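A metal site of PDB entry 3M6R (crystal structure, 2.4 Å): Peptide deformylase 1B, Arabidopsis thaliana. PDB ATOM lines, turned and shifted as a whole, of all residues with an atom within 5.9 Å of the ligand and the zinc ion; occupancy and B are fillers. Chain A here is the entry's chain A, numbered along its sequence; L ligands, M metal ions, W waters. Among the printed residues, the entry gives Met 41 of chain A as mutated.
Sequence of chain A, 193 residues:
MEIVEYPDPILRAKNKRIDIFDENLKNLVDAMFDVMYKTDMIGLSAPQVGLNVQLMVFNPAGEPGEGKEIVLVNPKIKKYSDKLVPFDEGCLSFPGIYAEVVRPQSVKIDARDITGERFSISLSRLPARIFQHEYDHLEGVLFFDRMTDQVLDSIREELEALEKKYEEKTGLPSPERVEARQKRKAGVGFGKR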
ATOM      1  N   THR A  39     -12.039  18.456 -25.885  1.00  0.00           N
ATOM      2  CA  THR A  39     -11.865  19.896 -25.752  1.00  0.00           C
ATOM      3  C   THR A  39     -10.664  20.259 -24.896  1.00  0.00           C
ATOM      4  O   THR A  39     -10.457  21.433 -24.591  1.00  0.00           O
ATOM      5  CB  THR A  39     -13.133  20.572 -25.161  1.00  0.00           C
ATOM      6  OG1 THR A  39     -13.407  20.036 -23.864  1.00  0.00           O
ATOM      7  CG2 THR A  39     -14.342  20.328 -26.071  1.00  0.00           C
ATOM      8  N   ASP A  40      -9.885  19.253 -24.522  1.00  0.00           N
ATOM      9  CA  ASP A  40      -8.694  19.455 -23.688  1.00  0.00           C
ATOM     10  C   ASP A  40      -8.972  20.082 -22.327  1.00  0.00           C
ATOM     11  O   ASP A  40      -8.182  20.897 -21.846  1.00  0.00           O
ATOM     12  CB  ASP A  40      -7.660  20.302 -24.433  1.00  0.00           C
ATOM     13  CG  ASP A  40      -6.585  19.468 -25.085  1.00  0.00           C
ATOM     14  OD1 ASP A  40      -6.893  18.739 -26.059  1.00  0.00           O
ATOM     15  OD2 ASP A  40      -5.431  19.526 -24.613  1.00  0.00           O
ATOM     16  N   MET A  41     -10.089  19.733 -21.708  1.00  0.00           N
ATOM     17  CA  MET A  41     -10.417  20.268 -20.397  1.00  0.00           C
ATOM     18  C   MET A  41     -10.056  19.218 -19.335  1.00  0.00           C
ATOM     19  O   MET A  41      -9.677  18.104 -19.668  1.00  0.00           O
ATOM     20  CB  MET A  41     -11.907  20.626 -20.323  1.00  0.00           C
ATOM     21  CG  MET A  41     -12.361  21.723 -21.302  1.00  0.00           C
ATOM     22  SD  MET A  41     -11.377  23.256 -21.299  1.00  0.00           S
ATOM     23  CE  MET A  41     -12.421  24.360 -20.722  1.00  0.00           C
ATOM     24  N   ILE A  42     -10.141  19.587 -18.062  1.00  0.00           N
ATOM     25  CA  ILE A  42      -9.831  18.613 -17.016  1.00  0.00           C
ATOM     26  C   ILE A  42     -11.066  18.301 -16.203  1.00  0.00           C
ATOM     27  O   ILE A  42     -11.009  17.523 -15.244  1.00  0.00           O
ATOM     28  CB  ILE A  42      -8.712  19.085 -16.069  1.00  0.00           C
ATOM     29  CG1 ILE A  42      -9.060  20.435 -15.450  1.00  0.00           C
ATOM     30  CG2 ILE A  42      -7.391  19.155 -16.830  1.00  0.00           C
ATOM     31  CD1 ILE A  42      -7.992  20.975 -14.530  1.00  0.00           C
ATOM     32  N   GLY A  43     -12.187  18.910 -16.602  1.00  0.00           N
ATOM     33  CA  GLY A  43     -13.450  18.695 -15.915  1.00  0.00           C
ATOM     34  C   GLY A  43     -14.623  19.169 -16.755  1.00  0.00           C
ATOM     35  O   GLY A  43     -14.425  19.845 -17.765  1.00  0.00           O
ATOM     36  N   LEU A  44     -15.832  18.837 -16.331  1.00  0.00           N
ATOM     37  CA  LEU A  44     -17.019  19.235 -17.080  1.00  0.00           C
ATOM     38  C   LEU A  44     -18.294  19.068 -16.254  1.00  0.00           C
ATOM     39  O   LEU A  44     -18.414  18.128 -15.459  1.00  0.00           O
ATOM     40  CB  LEU A  44     -17.105  18.407 -18.366  1.00  0.00           C
ATOM     41  CG  LEU A  44     -18.046  18.879 -19.464  1.00  0.00           C
ATOM     42  CD1 LEU A  44     -17.681  20.287 -19.905  1.00  0.00           C
ATOM     43  CD2 LEU A  44     -17.955  17.903 -20.630  1.00  0.00           C
ATOM     44  N   SER A  45     -19.233  19.981 -16.419  1.00  0.00           N
ATOM     45  CA  SER A  45     -20.502  19.892 -15.693  1.00  0.00           C
ATOM     46  C   SER A  45     -21.627  19.737 -16.717  1.00  0.00           C
ATOM     47  O   SER A  45     -21.462  20.076 -17.883  1.00  0.00           O
ATOM     48  CB  SER A  45     -20.742  21.126 -14.815  1.00  0.00           C
ATOM     49  OG  SER A  45     -20.926  22.300 -15.598  1.00  0.00           O
ATOM     50  N   GLN A  48     -23.046  22.631 -19.151  1.00  0.00           N
ATOM     51  CA  GLN A  48     -22.180  22.960 -20.262  1.00  0.00           C
ATOM     52  C   GLN A  48     -22.442  22.169 -21.532  1.00  0.00           C
ATOM     53  O   GLN A  48     -21.951  22.518 -22.617  1.00  0.00           O
ATOM     54  CB  GLN A  48     -20.727  22.816 -19.818  1.00  0.00           C
ATOM     55  CG  GLN A  48     -20.351  23.816 -18.749  1.00  0.00           C
ATOM     56  CD  GLN A  48     -18.948  23.623 -18.228  1.00  0.00           C
ATOM     57  OE1 GLN A  48     -18.701  22.730 -17.429  1.00  0.00           O
ATOM     58  NE2 GLN A  48     -18.022  24.456 -18.704  1.00  0.00           N
ATOM     59  N   PHE A  87      -5.310  30.815  -7.961  1.00  0.00           N
ATOM     60  CA  PHE A  87      -4.977  29.876  -9.026  1.00  0.00           C
ATOM     61  C   PHE A  87      -5.643  30.342 -10.324  1.00  0.00           C
ATOM     62  O   PHE A  87      -6.777  30.816 -10.317  1.00  0.00           O
ATOM     63  CB  PHE A  87      -5.435  28.472  -8.619  1.00  0.00           C
ATOM     64  CG  PHE A  87      -4.838  27.379  -9.450  1.00  0.00           C
ATOM     65  CD1 PHE A  87      -5.586  26.758 -10.442  1.00  0.00           C
ATOM     66  CD2 PHE A  87      -3.523  26.979  -9.256  1.00  0.00           C
ATOM     67  CE1 PHE A  87      -5.019  25.748 -11.238  1.00  0.00           C
ATOM     68  CE2 PHE A  87      -2.947  25.979 -10.041  1.00  0.00           C
ATOM     69  CZ  PHE A  87      -3.706  25.368 -11.041  1.00  0.00           C
ATOM     70  N   ASP A  88      -4.940  30.234 -11.447  1.00  0.00           N
ATOM     71  CA  ASP A  88      -5.498  30.658 -12.717  1.00  0.00           C
ATOM     72  C   ASP A  88      -6.461  29.616 -13.260  1.00  0.00           C
ATOM     73  O   ASP A  88      -6.194  28.409 -13.205  1.00  0.00           O
ATOM     74  CB  ASP A  88      -4.399  30.935 -13.750  1.00  0.00           C
ATOM     75  CG  ASP A  88      -3.606  32.192 -13.429  1.00  0.00           C
ATOM     76  OD1 ASP A  88      -4.224  33.211 -13.074  1.00  0.00           O
ATOM     77  OD2 ASP A  88      -2.355  32.159 -13.564  1.00  0.00           O
ATOM     78  N   GLU A  89      -7.590  30.091 -13.789  1.00  0.00           N
ATOM     79  CA  GLU A  89      -8.624  29.209 -14.304  1.00  0.00           C
ATOM     80  C   GLU A  89      -9.117  29.567 -15.689  1.00  0.00           C
ATOM     81  O   GLU A  89      -9.162  30.741 -16.077  1.00  0.00           O
ATOM     82  CB  GLU A  89      -9.834  29.199 -13.379  1.00  0.00           C
ATOM     83  CG  GLU A  89      -9.711  28.410 -12.092  1.00  0.00           C
ATOM     84  CD  GLU A  89     -10.944  28.548 -11.215  1.00  0.00           C
ATOM     85  OE1 GLU A  89     -12.076  28.525 -11.764  1.00  0.00           O
ATOM     86  OE2 GLU A  89     -10.807  28.686  -9.979  1.00  0.00           O
ATOM     87  N   GLY A  90      -9.515  28.536 -16.428  1.00  0.00           N
ATOM     88  CA  GLY A  90     -10.104  28.728 -17.740  1.00  0.00           C
ATOM     89  C   GLY A  90     -11.500  28.113 -17.627  1.00  0.00           C
ATOM     90  O   GLY A  90     -11.821  27.538 -16.585  1.00  0.00           O
ATOM     91  N   CYS A  91     -12.340  28.239 -18.649  1.00  0.00           N
ATOM     92  CA  CYS A  91     -13.683  27.638 -18.649  1.00  0.00           C
ATOM     93  C   CYS A  91     -14.161  27.415 -20.088  1.00  0.00           C
ATOM     94  O   CYS A  91     -14.141  28.339 -20.929  1.00  0.00           O
ATOM     95  CB  CYS A  91     -14.679  28.526 -17.883  1.00  0.00           C
ATOM     96  SG  CYS A  91     -16.410  27.867 -17.695  1.00  0.00           S
ATOM     97  N   LEU A  92     -14.573  26.192 -20.377  1.00  0.00           N
ATOM     98  CA  LEU A  92     -15.065  25.816 -21.694  1.00  0.00           C
ATOM     99  C   LEU A  92     -16.254  26.688 -22.143  1.00  0.00           C
ATOM    100  O   LEU A  92     -16.524  26.802 -23.334  1.00  0.00           O
ATOM    101  CB  LEU A  92     -15.481  24.344 -21.684  1.00  0.00           C
ATOM    102  CG  LEU A  92     -16.044  23.686 -22.946  1.00  0.00           C
ATOM    103  CD1 LEU A  92     -14.966  23.582 -24.041  1.00  0.00           C
ATOM    104  CD2 LEU A  92     -16.546  22.302 -22.575  1.00  0.00           C
ATOM    105  N   SER A  93     -16.954  27.314 -21.210  1.00  0.00           N
ATOM    106  CA  SER A  93     -18.083  28.143 -21.588  1.00  0.00           C
ATOM    107  C   SER A  93     -17.689  29.591 -21.934  1.00  0.00           C
ATOM    108  O   SER A  93     -18.503  30.374 -22.419  1.00  0.00           O
ATOM    109  CB  SER A  93     -19.151  28.106 -20.493  1.00  0.00           C
ATOM    110  OG  SER A  93     -19.608  26.780 -20.268  1.00  0.00           O
ATOM    111  N   TYR A  98      -8.822  33.614 -19.445  1.00  0.00           N
ATOM    112  CA  TYR A  98      -8.080  33.051 -18.317  1.00  0.00           C
ATOM    113  C   TYR A  98      -7.875  34.122 -17.257  1.00  0.00           C
ATOM    114  O   TYR A  98      -7.538  35.261 -17.562  1.00  0.00           O
ATOM    115  CB  TYR A  98      -6.707  32.548 -18.738  1.00  0.00           C
ATOM    116  CG  TYR A  98      -6.752  31.497 -19.795  1.00  0.00           C
ATOM    117  CD1 TYR A  98      -6.428  30.171 -19.508  1.00  0.00           C
ATOM    118  CD2 TYR A  98      -7.098  31.834 -21.112  1.00  0.00           C
ATOM    119  CE1 TYR A  98      -6.450  29.188 -20.516  1.00  0.00           C
ATOM    120  CE2 TYR A  98      -7.122  30.862 -22.129  1.00  0.00           C
ATOM    121  CZ  TYR A  98      -6.800  29.552 -21.819  1.00  0.00           C
ATOM    122  OH  TYR A  98      -6.827  28.610 -22.831  1.00  0.00           O
ATOM    123  N   ARG A 103      -9.964  30.622  -4.152  1.00  0.00           N
ATOM    124  CA  ARG A 103     -10.931  29.647  -3.652  1.00  0.00           C
ATOM    125  C   ARG A 103     -10.332  28.980  -2.428  1.00  0.00           C
ATOM    126  O   ARG A 103      -9.132  29.061  -2.209  1.00  0.00           O
ATOM    127  CB  ARG A 103     -11.222  28.544  -4.701  1.00  0.00           C
ATOM    128  CG  ARG A 103     -11.992  28.971  -5.968  1.00  0.00           C
ATOM    129  CD  ARG A 103     -12.184  27.772  -6.905  1.00  0.00           C
ATOM    130  NE  ARG A 103     -12.694  28.120  -8.240  1.00  0.00           N
ATOM    131  CZ  ARG A 103     -13.973  28.367  -8.539  1.00  0.00           C
ATOM    132  NH1 ARG A 103     -14.311  28.664  -9.791  1.00  0.00           N
ATOM    133  NH2 ARG A 103     -14.905  28.321  -7.606  1.00  0.00           N
ATOM    134  N   LEU A 126      -5.203  20.447  -6.504  1.00  0.00           N
ATOM    135  CA  LEU A 126      -5.913  20.584  -7.755  1.00  0.00           C
ATOM    136  C   LEU A 126      -7.313  19.944  -7.818  1.00  0.00           C
ATOM    137  O   LEU A 126      -8.254  20.517  -8.375  1.00  0.00           O
ATOM    138  CB  LEU A 126      -5.044  20.062  -8.896  1.00  0.00           C
ATOM    139  CG  LEU A 126      -5.623  20.229 -10.303  1.00  0.00           C
ATOM    140  CD1 LEU A 126      -5.828  21.714 -10.596  1.00  0.00           C
ATOM    141  CD2 LEU A 126      -4.685  19.606 -11.321  1.00  0.00           C
ATOM    142  N   ARG A 129      -9.754  22.124  -6.514  1.00  0.00           N
ATOM    143  CA  ARG A 129      -9.907  23.273  -7.374  1.00  0.00           C
ATOM    144  C   ARG A 129     -10.933  23.038  -8.455  1.00  0.00           C
ATOM    145  O   ARG A 129     -11.796  23.882  -8.706  1.00  0.00           O
ATOM    146  CB  ARG A 129      -8.597  23.588  -8.070  1.00  0.00           C
ATOM    147  CG  ARG A 129      -8.674  24.904  -8.758  1.00  0.00           C
ATOM    148  CD  ARG A 129      -8.832  25.902  -7.666  1.00  0.00           C
ATOM    149  NE  ARG A 129      -9.144  27.213  -8.179  1.00  0.00           N
ATOM    150  CZ  ARG A 129      -8.833  28.330  -7.544  1.00  0.00           C
ATOM    151  NH1 ARG A 129      -8.198  28.268  -6.379  1.00  0.00           N
ATOM    152  NH2 ARG A 129      -9.146  29.485  -8.099  1.00  0.00           N
ATOM    153  N   ILE A 130     -10.797  21.892  -9.122  1.00  0.00           N
ATOM    154  CA  ILE A 130     -11.665  21.462 -10.201  1.00  0.00           C
ATOM    155  C   ILE A 130     -13.089  21.252  -9.685  1.00  0.00           C
ATOM    156  O   ILE A 130     -14.042  21.773 -10.239  1.00  0.00           O
ATOM    157  CB  ILE A 130     -11.148  20.133 -10.817  1.00  0.00           C
ATOM    158  CG1 ILE A 130      -9.706  20.297 -11.280  1.00  0.00           C
ATOM    159  CG2 ILE A 130     -12.030  19.704 -11.976  1.00  0.00           C
ATOM    160  CD1 ILE A 130      -9.078  18.998 -11.797  1.00  0.00           C
ATOM    161  N   HIS A 133     -14.987  24.502  -9.064  1.00  0.00           N
ATOM    162  CA  HIS A 133     -15.328  25.203 -10.289  1.00  0.00           C
ATOM    163  C   HIS A 133     -16.612  24.574 -10.873  1.00  0.00           C
ATOM    164  O   HIS A 133     -17.525  25.277 -11.313  1.00  0.00           O
ATOM    165  CB  HIS A 133     -14.181  25.063 -11.292  1.00  0.00           C
ATOM    166  CG  HIS A 133     -14.431  25.728 -12.609  1.00  0.00           C
ATOM    167  ND1 HIS A 133     -14.290  27.088 -12.789  1.00  0.00           N
ATOM    168  CD2 HIS A 133     -14.809  25.226 -13.799  1.00  0.00           C
ATOM    169  CE1 HIS A 133     -14.557  27.385 -14.045  1.00  0.00           C
ATOM    170  NE2 HIS A 133     -14.879  26.276 -14.678  1.00  0.00           N
ATOM    171  N   GLU A 134     -16.662  23.240 -10.857  1.00  0.00           N
ATOM    172  CA  GLU A 134     -17.806  22.488 -11.377  1.00  0.00           C
ATOM    173  C   GLU A 134     -19.020  22.652 -10.457  1.00  0.00           C
ATOM    174  O   GLU A 134     -20.134  22.902 -10.908  1.00  0.00           O
ATOM    175  CB  GLU A 134     -17.439  21.012 -11.488  1.00  0.00           C
ATOM    176  CG  GLU A 134     -16.109  20.745 -12.167  1.00  0.00           C
ATOM    177  CD  GLU A 134     -16.072  21.193 -13.624  1.00  0.00           C
ATOM    178  OE1 GLU A 134     -14.953  21.328 -14.171  1.00  0.00           O
ATOM    179  OE2 GLU A 134     -17.146  21.390 -14.226  1.00  0.00           O
ATOM    180  N   HIS A 137     -20.698  25.579 -11.099  1.00  0.00           N
ATOM    181  CA  HIS A 137     -21.490  25.371 -12.293  1.00  0.00           C
ATOM    182  C   HIS A 137     -22.858  24.760 -11.980  1.00  0.00           C
ATOM    183  O   HIS A 137     -23.883  25.232 -12.475  1.00  0.00           O
ATOM    184  CB  HIS A 137     -20.761  24.449 -13.270  1.00  0.00           C
ATOM    185  CG  HIS A 137     -19.995  25.156 -14.331  1.00  0.00           C
ATOM    186  ND1 HIS A 137     -20.599  25.946 -15.294  1.00  0.00           N
ATOM    187  CD2 HIS A 137     -18.665  25.166 -14.616  1.00  0.00           C
ATOM    188  CE1 HIS A 137     -19.678  26.404 -16.127  1.00  0.00           C
ATOM    189  NE2 HIS A 137     -18.496  25.937 -15.732  1.00  0.00           N
HETATM  190  C1  LIG L   1     -13.287  23.135 -17.785  1.00  0.00           C
HETATM  191  C2  LIG L   1     -14.714  23.386 -17.082  1.00  0.00           C
HETATM  192  O1  LIG L   1     -15.051  24.396 -17.717  1.00  0.00           O
HETATM  193  N1  LIG L   1     -15.520  22.849 -16.166  1.00  0.00           N
HETATM  194  O2  LIG L   1     -16.739  23.441 -15.863  1.00  0.00           O
HETATM  195  C3  LIG L   1     -12.293  23.931 -16.865  1.00  0.00           C
HETATM  196  C4  LIG L   1     -10.921  23.641 -17.559  1.00  0.00           C
HETATM  197  O3  LIG L   1     -10.622  22.466 -17.826  1.00  0.00           O
HETATM  198  C5  LIG L   1     -12.289  23.319 -15.434  1.00  0.00           C
HETATM  199  C6  LIG L   1     -11.316  24.172 -14.575  1.00  0.00           C
HETATM  200  C7  LIG L   1     -11.179  23.692 -13.164  1.00  0.00           C
HETATM  201  C8  LIG L   1     -10.391  24.752 -12.416  1.00  0.00           C
HETATM  202  C9  LIG L   1      -8.892  24.522 -12.584  1.00  0.00           C
HETATM  203  N2  LIG L   1     -10.210  24.805 -17.773  1.00  0.00           N
HETATM  204  C10 LIG L   1      -8.763  24.460 -17.630  1.00  0.00           C
HETATM  205  C11 LIG L   1      -8.128  24.914 -19.023  1.00  0.00           C
HETATM  206  C12 LIG L   1      -8.315  23.844 -20.134  1.00  0.00           C
HETATM  207  C13 LIG L   1      -8.729  26.270 -19.541  1.00  0.00           C
HETATM  208  C14 LIG L   1      -8.030  25.239 -16.483  1.00  0.00           C
HETATM  209  O4  LIG L   1      -8.631  26.076 -15.851  1.00  0.00           O
HETATM  210  N3  LIG L   1      -6.598  24.616 -16.399  1.00  0.00           N
HETATM  211  C15 LIG L   1      -5.642  25.125 -15.366  1.00  0.00           C
HETATM  212  C16 LIG L   1      -5.876  23.517 -17.147  1.00  0.00           C
HETATM  213  C17 LIG L   1      -4.868  22.972 -16.115  1.00  0.00           C
HETATM  214  C18 LIG L   1      -4.345  24.297 -15.525  1.00  0.00           C
HETATM  215  C19 LIG L   1      -5.319  26.618 -15.599  1.00  0.00           C
HETATM  216  O5  LIG L   1      -4.422  27.105 -14.605  1.00  0.00           O
HETATM  217 ZN    ZN M   1     -16.314  25.897 -16.311  1.00  0.00          ZN
HETATM  218  O   HOH W   1      -3.214  29.240 -17.061  1.00  0.00           O
HETATM  219  O   HOH W   2      -1.408  23.141 -16.168  1.00  0.00           O
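O3 of the ligand lies close to SD of Met 41.
Asp 40 touches the ligand.
Gly 43 touches the ligand.
Phe 87 touches the ligand.
CA of Glu 89 touches O4 of the ligand, 3.5 Å away.
Tyr 98 touches the ligand.
Arg 129 touches the ligand (CG to C9, 3.9 Å).
CA of Ile 130 touches C7 of the ligand, 3.7 Å away.
Hydrophobic or aromatic side chains within 4 Å of the ligand: Met 41, Ile 42, Phe 87, Leu 92, Tyr 98, His 133 and His 137.
Within 4 Å of the ligand: Asp 40, Met 41, Ile 42, Gly 43, Gln 48, Phe 87, Asp 88, Glu 89, Gly 90, Cys 91, Leu 92, Tyr 98, Arg 129, Ile 130, His 133, Glu 134 and His 137.
The nearest printed residue that does not touch the ligand is Leu 44 (4.02 Å).
A ring nitrogen (ND1) of His 133 sits at hydrogen-bond distance from the side-chain carboxylate (OE1) of Glu 89 (2.8 Å).
OE1 of Glu 134 sits at hydrogen-bond distance from N of Leu 44, 3.4 Å away.
The side-chain carboxylate (OE2) of Glu 89 is in salt-bridge range of the guanidinium group (NH2) of Arg 129 (2.6 Å).
ND1 of His 133 lies within hydrogen-bond range of NH1 of Arg 103 (3.4 Å).
A ring nitrogen (NE2) of His 137 lies close to the side-chain amide nitrogen (NE2) of Gln 48 (3.4 Å).
The side-chain sulfur of Cys 91 lies close to the backbone NH of Ser 93 (3.6 Å).
The guanidinium group (NE) of Arg 103 is in salt-bridge range of the side-chain carboxylate (OE2) of Glu 89 (2.6 Å).
NE2 of Gln 48 sits at hydrogen-bond distance from OG of Ser 93 (3.2 Å).
Residues that only touch the zinc ion: Gln 48 (3.3 Å).
Of the 23 residues printed, 4 come within 4 Å of the zinc ion.
The nearest printed residue that does not touch the zinc ion is Leu 92 (4.4 Å).
The zinc ion is bound by NE2 of His 133 (2.2 Å), NE2 of His 137 (2.3 Å), SG of Cys 91 (2.4 Å), O1 of the ligand (2.4 Å) and O2 of the ligand (2.5 Å).
The zinc ion has five donor atoms within binding distance.
A nitrogen (N1) of the ligand sits at hydrogen-bond distance from the side-chain carboxylate (OE1) of Glu 134, 2.6 Å away.
The backbone carbonyl oxygen (O) of Gly 90 lies within hydrogen-bond range of a nitrogen (N2) of the ligand (3.4 Å).
The backbone NH (N) of Gly 90 is in hydrogen-bond range of an oxygen (O4) of the ligand.
O of Asp 88 lies within hydrogen-bond range of O5 of the ligand.
A nitrogen (N1) of the ligand lies within hydrogen-bond range of the side-chain amide oxygen of Gln 48, 3.4 Å away.
N of Leu 92 sits close to O1 of the ligand, at 3.2 Å.
The backbone NH of Ile 42 sits at hydrogen-bond distance from an oxygen (O3) of the ligand (2.9 Å).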
